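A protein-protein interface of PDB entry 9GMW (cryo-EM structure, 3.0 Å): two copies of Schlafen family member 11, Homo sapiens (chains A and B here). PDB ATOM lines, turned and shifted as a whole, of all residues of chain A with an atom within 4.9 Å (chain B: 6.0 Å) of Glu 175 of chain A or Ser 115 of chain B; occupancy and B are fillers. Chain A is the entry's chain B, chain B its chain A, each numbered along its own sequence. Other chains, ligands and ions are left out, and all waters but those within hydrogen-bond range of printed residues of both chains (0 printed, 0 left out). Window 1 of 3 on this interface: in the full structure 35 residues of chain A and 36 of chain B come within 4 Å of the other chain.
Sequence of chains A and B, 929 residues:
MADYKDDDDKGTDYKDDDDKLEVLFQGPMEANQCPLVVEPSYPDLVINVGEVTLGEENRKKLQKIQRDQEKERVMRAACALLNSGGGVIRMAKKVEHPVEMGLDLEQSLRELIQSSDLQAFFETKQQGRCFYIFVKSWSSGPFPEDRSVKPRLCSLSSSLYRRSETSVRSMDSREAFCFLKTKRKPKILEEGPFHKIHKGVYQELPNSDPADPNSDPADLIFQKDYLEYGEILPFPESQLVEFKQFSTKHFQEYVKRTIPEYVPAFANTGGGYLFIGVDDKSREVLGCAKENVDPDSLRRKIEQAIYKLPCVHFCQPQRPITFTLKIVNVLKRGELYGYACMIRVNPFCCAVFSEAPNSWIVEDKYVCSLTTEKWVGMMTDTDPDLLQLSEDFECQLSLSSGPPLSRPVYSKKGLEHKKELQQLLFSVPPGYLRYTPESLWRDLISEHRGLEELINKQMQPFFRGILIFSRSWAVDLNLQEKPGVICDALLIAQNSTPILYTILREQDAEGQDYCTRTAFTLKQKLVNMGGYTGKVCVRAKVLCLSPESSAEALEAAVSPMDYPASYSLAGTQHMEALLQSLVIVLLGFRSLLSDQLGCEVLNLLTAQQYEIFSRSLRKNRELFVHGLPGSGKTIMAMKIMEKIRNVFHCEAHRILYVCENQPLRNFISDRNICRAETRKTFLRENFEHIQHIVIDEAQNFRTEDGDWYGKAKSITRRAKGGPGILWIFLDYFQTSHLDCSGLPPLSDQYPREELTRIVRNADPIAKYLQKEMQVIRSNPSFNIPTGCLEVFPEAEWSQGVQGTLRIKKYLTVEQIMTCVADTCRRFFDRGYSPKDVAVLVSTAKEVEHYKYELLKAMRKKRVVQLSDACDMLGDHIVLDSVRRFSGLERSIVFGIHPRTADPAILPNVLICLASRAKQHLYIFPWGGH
NE of Arg 162 of chain A sits at hydrogen-bond distance from OG of Ser 116 of chain B (2.8 Å).
The side-chain carboxylate of Glu 175 of chain A is in hydrogen-bond range of the side-chain hydroxyl of Ser 116 of chain B.
The side-chain carboxylate (OD2) of Asp 117 of chain B lies within salt-bridge range of the guanidinium group (NH1) of Arg 162 of chain A (3.8 Å).
The backbone carbonyl oxygen (O) of Arg 110 of chain B is in hydrogen-bond range of the backbone NH (N) of Ser 115 of chain B, at 3.2 Å.
OG of Ser 115 of chain B is in hydrogen-bond range of N of Asp 117 of chain B, 3.1 Å away.
The guanidinium group (NH2) of Arg 162 of chain A is in salt-bridge range of the side-chain carboxylate (OE1) of Glu 175 of chain A.
OD2 of Asp 172 of chain A lies within hydrogen-bond range of N of Glu 175 of chain A.
Among the printed residues, merely in contact across the chains: Arg 162 of chain A with Ser 115 of chain B (3.8 Å) and Glu 175 of chain A with Ser 115 of chain B (3.8 Å).
Of the printed residues of chain B, Arg 162 of chain A touches Ser 115 (3.8 Å), Ser 116 (2.8 Å) and Asp 117 (3.7 Å).
Ser 170 of chain A touches none of the printed residues of chain B.
Glu 175 of chain A touches two residues of chain B.
Phe 179 of chain A touches none of the printed residues of chain B.
Of chain A, only Arg 162 and Glu 175 come within 4 Å of Ser 115 of chain B.
Printed residues of chain A within 4 Å of Ser 116 of chain B: Arg 162 (2.8 Å) and Glu 175 (2.9 Å).
Of the printed residues of chain A, Asp 117 of chain B touches Arg 162.
The nearest residue of chain B that does not touch Glu 175 of chain A is Asp 117 of chain B (4.6 Å).
The nearest printed residue of chain A that does not touch Ser 115 of chain B is Asp 172 of chain A (6.2 Å).
Of the 11 printed residues of chain A, 2 touch a printed residue of chain B.
Among the printed residues, 5 pairs touch across the chains.
Among the printed residues, Asp or Glu carboxylates within 4 Å of a Lys or Arg side-chain nitrogen of the other chain: Arg 162 of chain A with Asp 117 of chain B (3.8 Å).
No position is printed for both chains.
Of the 5 pairs that touch across the chains among the printed residues, none has its exchanged pair printed and touching as well.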
ATOM      1  N   ARG A 162       7.645 -23.840  14.968  1.00  0.00           N
ATOM      2  CA  ARG A 162       6.372 -24.427  14.583  1.00  0.00           C
ATOM      3  C   ARG A 162       5.919 -23.852  13.252  1.00  0.00           C
ATOM      4  O   ARG A 162       6.182 -22.691  12.935  1.00  0.00           O
ATOM      5  CB  ARG A 162       5.287 -24.189  15.635  1.00  0.00           C
ATOM      6  CG  ARG A 162       4.958 -22.735  15.909  1.00  0.00           C
ATOM      7  CD  ARG A 162       3.608 -22.634  16.589  1.00  0.00           C
ATOM      8  NE  ARG A 162       3.587 -21.628  17.644  1.00  0.00           N
ATOM      9  CZ  ARG A 162       2.981 -21.774  18.814  1.00  0.00           C
ATOM     10  NH1 ARG A 162       2.329 -22.882  19.126  1.00  0.00           N
ATOM     11  NH2 ARG A 162       3.028 -20.782  19.696  1.00  0.00           N
ATOM     12  N   SER A 170       9.791 -18.898  15.029  1.00  0.00           N
ATOM     13  CA  SER A 170      10.410 -19.256  16.295  1.00  0.00           C
ATOM     14  C   SER A 170       9.529 -18.798  17.449  1.00  0.00           C
ATOM     15  O   SER A 170       8.974 -17.696  17.417  1.00  0.00           O
ATOM     16  CB  SER A 170      11.792 -18.617  16.407  1.00  0.00           C
ATOM     17  OG  SER A 170      12.459 -19.038  17.584  1.00  0.00           O
ATOM     18  N   MET A 171       9.402 -19.644  18.466  1.00  0.00           N
ATOM     19  CA  MET A 171       8.621 -19.296  19.643  1.00  0.00           C
ATOM     20  C   MET A 171       9.467 -18.452  20.584  1.00  0.00           C
ATOM     21  O   MET A 171      10.566 -18.860  20.971  1.00  0.00           O
ATOM     22  CB  MET A 171       8.144 -20.557  20.354  1.00  0.00           C
ATOM     23  CG  MET A 171       7.209 -21.423  19.545  1.00  0.00           C
ATOM     24  SD  MET A 171       6.594 -22.819  20.496  1.00  0.00           S
ATOM     25  CE  MET A 171       6.659 -24.118  19.274  1.00  0.00           C
ATOM     26  N   ASP A 172       8.962 -17.281  20.955  1.00  0.00           N
ATOM     27  CA  ASP A 172       9.617 -16.478  21.974  1.00  0.00           C
ATOM     28  C   ASP A 172       9.458 -17.163  23.328  1.00  0.00           C
ATOM     29  O   ASP A 172       8.950 -18.279  23.431  1.00  0.00           O
ATOM     30  CB  ASP A 172       9.049 -15.063  21.981  1.00  0.00           C
ATOM     31  CG  ASP A 172       7.542 -15.044  22.029  1.00  0.00           C
ATOM     32  OD1 ASP A 172       6.916 -15.069  20.951  1.00  0.00           O
ATOM     33  OD2 ASP A 172       6.979 -15.021  23.141  1.00  0.00           O
ATOM     34  N   SER A 173       9.926 -16.505  24.388  1.00  0.00           N
ATOM     35  CA  SER A 173       9.889 -17.142  25.698  1.00  0.00           C
ATOM     36  C   SER A 173       8.456 -17.427  26.132  1.00  0.00           C
ATOM     37  O   SER A 173       8.160 -18.516  26.628  1.00  0.00           O
ATOM     38  CB  SER A 173      10.606 -16.274  26.731  1.00  0.00           C
ATOM     39  OG  SER A 173      11.905 -15.929  26.290  1.00  0.00           O
ATOM     40  N   ARG A 174       7.550 -16.467  25.938  1.00  0.00           N
ATOM     41  CA  ARG A 174       6.155 -16.664  26.329  1.00  0.00           C
ATOM     42  C   ARG A 174       5.501 -17.776  25.515  1.00  0.00           C
ATOM     43  O   ARG A 174       4.804 -18.639  26.067  1.00  0.00           O
ATOM     44  CB  ARG A 174       5.392 -15.355  26.150  1.00  0.00           C
ATOM     45  CG  ARG A 174       3.939 -15.397  26.564  1.00  0.00           C
ATOM     46  CD  ARG A 174       3.343 -14.001  26.578  1.00  0.00           C
ATOM     47  NE  ARG A 174       3.940 -13.155  27.606  1.00  0.00           N
ATOM     48  CZ  ARG A 174       4.786 -12.159  27.374  1.00  0.00           C
ATOM     49  NH1 ARG A 174       5.205 -11.873  26.151  1.00  0.00           N
ATOM     50  NH2 ARG A 174       5.229 -11.432  28.396  1.00  0.00           N
ATOM     51  N   GLU A 175       5.714 -17.766  24.198  1.00  0.00           N
ATOM     52  CA  GLU A 175       5.133 -18.790  23.338  1.00  0.00           C
ATOM     53  C   GLU A 175       5.656 -20.170  23.699  1.00  0.00           C
ATOM     54  O   GLU A 175       4.892 -21.138  23.753  1.00  0.00           O
ATOM     55  CB  GLU A 175       5.450 -18.480  21.879  1.00  0.00           C
ATOM     56  CG  GLU A 175       4.569 -17.431  21.251  1.00  0.00           C
ATOM     57  CD  GLU A 175       4.701 -17.407  19.748  1.00  0.00           C
ATOM     58  OE1 GLU A 175       4.523 -18.471  19.120  1.00  0.00           O
ATOM     59  OE2 GLU A 175       5.004 -16.328  19.198  1.00  0.00           O
ATOM     60  N   ALA A 176       6.963 -20.281  23.936  1.00  0.00           N
ATOM     61  CA  ALA A 176       7.547 -21.565  24.298  1.00  0.00           C
ATOM     62  C   ALA A 176       7.066 -22.018  25.667  1.00  0.00           C
ATOM     63  O   ALA A 176       6.859 -23.212  25.891  1.00  0.00           O
ATOM     64  CB  ALA A 176       9.070 -21.478  24.268  1.00  0.00           C
ATOM     65  N   PHE A 177       6.892 -21.081  26.597  1.00  0.00           N
ATOM     66  CA  PHE A 177       6.355 -21.431  27.902  1.00  0.00           C
ATOM     67  C   PHE A 177       4.974 -22.048  27.765  1.00  0.00           C
ATOM     68  O   PHE A 177       4.704 -23.122  28.312  1.00  0.00           O
ATOM     69  CB  PHE A 177       6.309 -20.189  28.789  1.00  0.00           C
ATOM     70  CG  PHE A 177       5.699 -20.427  30.135  1.00  0.00           C
ATOM     71  CD1 PHE A 177       6.248 -21.348  31.005  1.00  0.00           C
ATOM     72  CD2 PHE A 177       4.581 -19.723  30.532  1.00  0.00           C
ATOM     73  CE1 PHE A 177       5.687 -21.565  32.241  1.00  0.00           C
ATOM     74  CE2 PHE A 177       4.020 -19.938  31.766  1.00  0.00           C
ATOM     75  CZ  PHE A 177       4.574 -20.859  32.622  1.00  0.00           C
ATOM     76  N   CYS A 178       4.087 -21.386  27.018  1.00  0.00           N
ATOM     77  CA  CYS A 178       2.751 -21.938  26.814  1.00  0.00           C
ATOM     78  C   CYS A 178       2.798 -23.273  26.080  1.00  0.00           C
ATOM     79  O   CYS A 178       2.052 -24.197  26.422  1.00  0.00           O
ATOM     80  CB  CYS A 178       1.886 -20.941  26.050  1.00  0.00           C
ATOM     81  SG  CYS A 178       1.564 -19.413  26.954  1.00  0.00           S
ATOM     82  N   PHE A 179       3.663 -23.396  25.074  1.00  0.00           N
ATOM     83  CA  PHE A 179       3.757 -24.636  24.314  1.00  0.00           C
ATOM     84  C   PHE A 179       4.202 -25.795  25.198  1.00  0.00           C
ATOM     85  O   PHE A 179       3.620 -26.884  25.153  1.00  0.00           O
ATOM     86  CB  PHE A 179       4.721 -24.438  23.146  1.00  0.00           C
ATOM     87  CG  PHE A 179       5.101 -25.705  22.447  1.00  0.00           C
ATOM     88  CD1 PHE A 179       4.215 -26.336  21.599  1.00  0.00           C
ATOM     89  CD2 PHE A 179       6.354 -26.256  22.626  1.00  0.00           C
ATOM     90  CE1 PHE A 179       4.571 -27.496  20.954  1.00  0.00           C
ATOM     91  CE2 PHE A 179       6.710 -27.413  21.983  1.00  0.00           C
ATOM     92  CZ  PHE A 179       5.820 -28.033  21.148  1.00  0.00           C
ATOM     93  N   LEU B 109      -2.391 -11.403  10.724  1.00  0.00           N
ATOM     94  CA  LEU B 109      -3.106 -12.246  11.680  1.00  0.00           C
ATOM     95  C   LEU B 109      -2.224 -12.600  12.873  1.00  0.00           C
ATOM     96  O   LEU B 109      -2.698 -12.638  14.018  1.00  0.00           O
ATOM     97  CB  LEU B 109      -3.606 -13.514  10.991  1.00  0.00           C
ATOM     98  CG  LEU B 109      -4.632 -13.329   9.872  1.00  0.00           C
ATOM     99  CD1 LEU B 109      -5.034 -14.673   9.301  1.00  0.00           C
ATOM    100  CD2 LEU B 109      -5.852 -12.572  10.356  1.00  0.00           C
ATOM    101  N   ARG B 110      -0.944 -12.883  12.623  1.00  0.00           N
ATOM    102  CA  ARG B 110      -0.027 -13.178  13.719  1.00  0.00           C
ATOM    103  C   ARG B 110       0.101 -11.986  14.652  1.00  0.00           C
ATOM    104  O   ARG B 110       0.101 -12.146  15.875  1.00  0.00           O
ATOM    105  CB  ARG B 110       1.346 -13.564  13.177  1.00  0.00           C
ATOM    106  CG  ARG B 110       1.404 -14.929  12.547  1.00  0.00           C
ATOM    107  CD  ARG B 110       2.827 -15.312  12.213  1.00  0.00           C
ATOM    108  NE  ARG B 110       2.872 -16.345  11.187  1.00  0.00           N
ATOM    109  CZ  ARG B 110       3.140 -16.126   9.907  1.00  0.00           C
ATOM    110  NH1 ARG B 110       3.433 -14.919   9.454  1.00  0.00           N
ATOM    111  NH2 ARG B 110       3.113 -17.145   9.057  1.00  0.00           N
ATOM    112  N   GLU B 111       0.221 -10.782  14.095  1.00  0.00           N
ATOM    113  CA  GLU B 111       0.216  -9.588  14.929  1.00  0.00           C
ATOM    114  C   GLU B 111      -1.090  -9.461  15.691  1.00  0.00           C
ATOM    115  O   GLU B 111      -1.096  -9.046  16.853  1.00  0.00           O
ATOM    116  CB  GLU B 111       0.441  -8.341  14.075  1.00  0.00           C
ATOM    117  CG  GLU B 111       1.793  -8.271  13.397  1.00  0.00           C
ATOM    118  CD  GLU B 111       1.866  -7.151  12.375  1.00  0.00           C
ATOM    119  OE1 GLU B 111       2.608  -7.294  11.380  1.00  0.00           O
ATOM    120  OE2 GLU B 111       1.178  -6.127  12.565  1.00  0.00           O
ATOM    121  N   LEU B 112      -2.204  -9.806  15.049  1.00  0.00           N
ATOM    122  CA  LEU B 112      -3.515  -9.655  15.663  1.00  0.00           C
ATOM    123  C   LEU B 112      -3.653 -10.523  16.905  1.00  0.00           C
ATOM    124  O   LEU B 112      -4.140 -10.055  17.940  1.00  0.00           O
ATOM    125  CB  LEU B 112      -4.593 -10.000  14.636  1.00  0.00           C
ATOM    126  CG  LEU B 112      -6.024  -9.517  14.852  1.00  0.00           C
ATOM    127  CD1 LEU B 112      -6.063  -8.049  15.223  1.00  0.00           C
ATOM    128  CD2 LEU B 112      -6.824  -9.766  13.593  1.00  0.00           C
ATOM    129  N   ILE B 113      -3.214 -11.784  16.831  1.00  0.00           N
ATOM    130  CA  ILE B 113      -3.321 -12.677  17.983  1.00  0.00           C
ATOM    131  C   ILE B 113      -2.059 -12.704  18.837  1.00  0.00           C
ATOM    132  O   ILE B 113      -2.010 -13.448  19.826  1.00  0.00           O
ATOM    133  CB  ILE B 113      -3.676 -14.117  17.558  1.00  0.00           C
ATOM    134  CG1 ILE B 113      -2.637 -14.681  16.593  1.00  0.00           C
ATOM    135  CG2 ILE B 113      -5.051 -14.150  16.930  1.00  0.00           C
ATOM    136  CD1 ILE B 113      -2.736 -16.172  16.413  1.00  0.00           C
ATOM    137  N   GLN B 114      -1.043 -11.910  18.500  1.00  0.00           N
ATOM    138  CA  GLN B 114       0.221 -11.890  19.238  1.00  0.00           C
ATOM    139  C   GLN B 114       0.774 -13.297  19.427  1.00  0.00           C
ATOM    140  O   GLN B 114       1.191 -13.682  20.520  1.00  0.00           O
ATOM    141  CB  GLN B 114       0.073 -11.196  20.589  1.00  0.00           C
ATOM    142  CG  GLN B 114      -0.506  -9.805  20.531  1.00  0.00           C
ATOM    143  CD  GLN B 114      -1.038  -9.358  21.871  1.00  0.00           C
ATOM    144  OE1 GLN B 114      -0.519  -8.424  22.474  1.00  0.00           O
ATOM    145  NE2 GLN B 114      -2.074 -10.035  22.351  1.00  0.00           N
ATOM    146  N   SER B 115       0.779 -14.078  18.353  1.00  0.00           N
ATOM    147  CA  SER B 115       1.297 -15.435  18.424  1.00  0.00           C
ATOM    148  C   SER B 115       1.458 -15.979  17.017  1.00  0.00           C
ATOM    149  O   SER B 115       0.751 -15.571  16.095  1.00  0.00           O
ATOM    150  CB  SER B 115       0.372 -16.343  19.238  1.00  0.00           C
ATOM    151  OG  SER B 115       0.860 -17.672  19.267  1.00  0.00           O
ATOM    152  N   SER B 116       2.402 -16.907  16.865  1.00  0.00           N
ATOM    153  CA  SER B 116       2.550 -17.627  15.610  1.00  0.00           C
ATOM    154  C   SER B 116       1.579 -18.791  15.495  1.00  0.00           C
ATOM    155  O   SER B 116       1.538 -19.440  14.446  1.00  0.00           O
ATOM    156  CB  SER B 116       3.984 -18.134  15.465  1.00  0.00           C
ATOM    157  OG  SER B 116       4.252 -19.185  16.374  1.00  0.00           O
ATOM    158  N   ASP B 117       0.806 -19.070  16.545  1.00  0.00           N
ATOM    159  CA  ASP B 117      -0.171 -20.156  16.544  1.00  0.00           C
ATOM    160  C   ASP B 117      -1.481 -19.687  15.908  1.00  0.00           C
ATOM    161  O   ASP B 117      -2.478 -19.416  16.577  1.00  0.00           O
ATOM    162  CB  ASP B 117      -0.395 -20.650  17.967  1.00  0.00           C
ATOM    163  CG  ASP B 117      -1.054 -22.009  18.019  1.00  0.00           C
ATOM    164  OD1 ASP B 117      -1.198 -22.646  16.959  1.00  0.00           O
ATOM    165  OD2 ASP B 117      -1.429 -22.443  19.127  1.00  0.00           O
ATOM    166  N   LEU B 118      -1.457 -19.582  14.580  1.00  0.00           N
ATOM    167  CA  LEU B 118      -2.651 -19.164  13.856  1.00  0.00           C
ATOM    168  C   LEU B 118      -3.729 -20.235  13.917  1.00  0.00           C
ATOM    169  O   LEU B 118      -4.919 -19.920  14.001  1.00  0.00           O
ATOM    170  CB  LEU B 118      -2.297 -18.842  12.404  1.00  0.00           C
ATOM    171  CG  LEU B 118      -1.390 -17.635  12.158  1.00  0.00           C
ATOM    172  CD1 LEU B 118      -1.100 -17.496  10.681  1.00  0.00           C
ATOM    173  CD2 LEU B 118      -2.006 -16.365  12.693  1.00  0.00           C
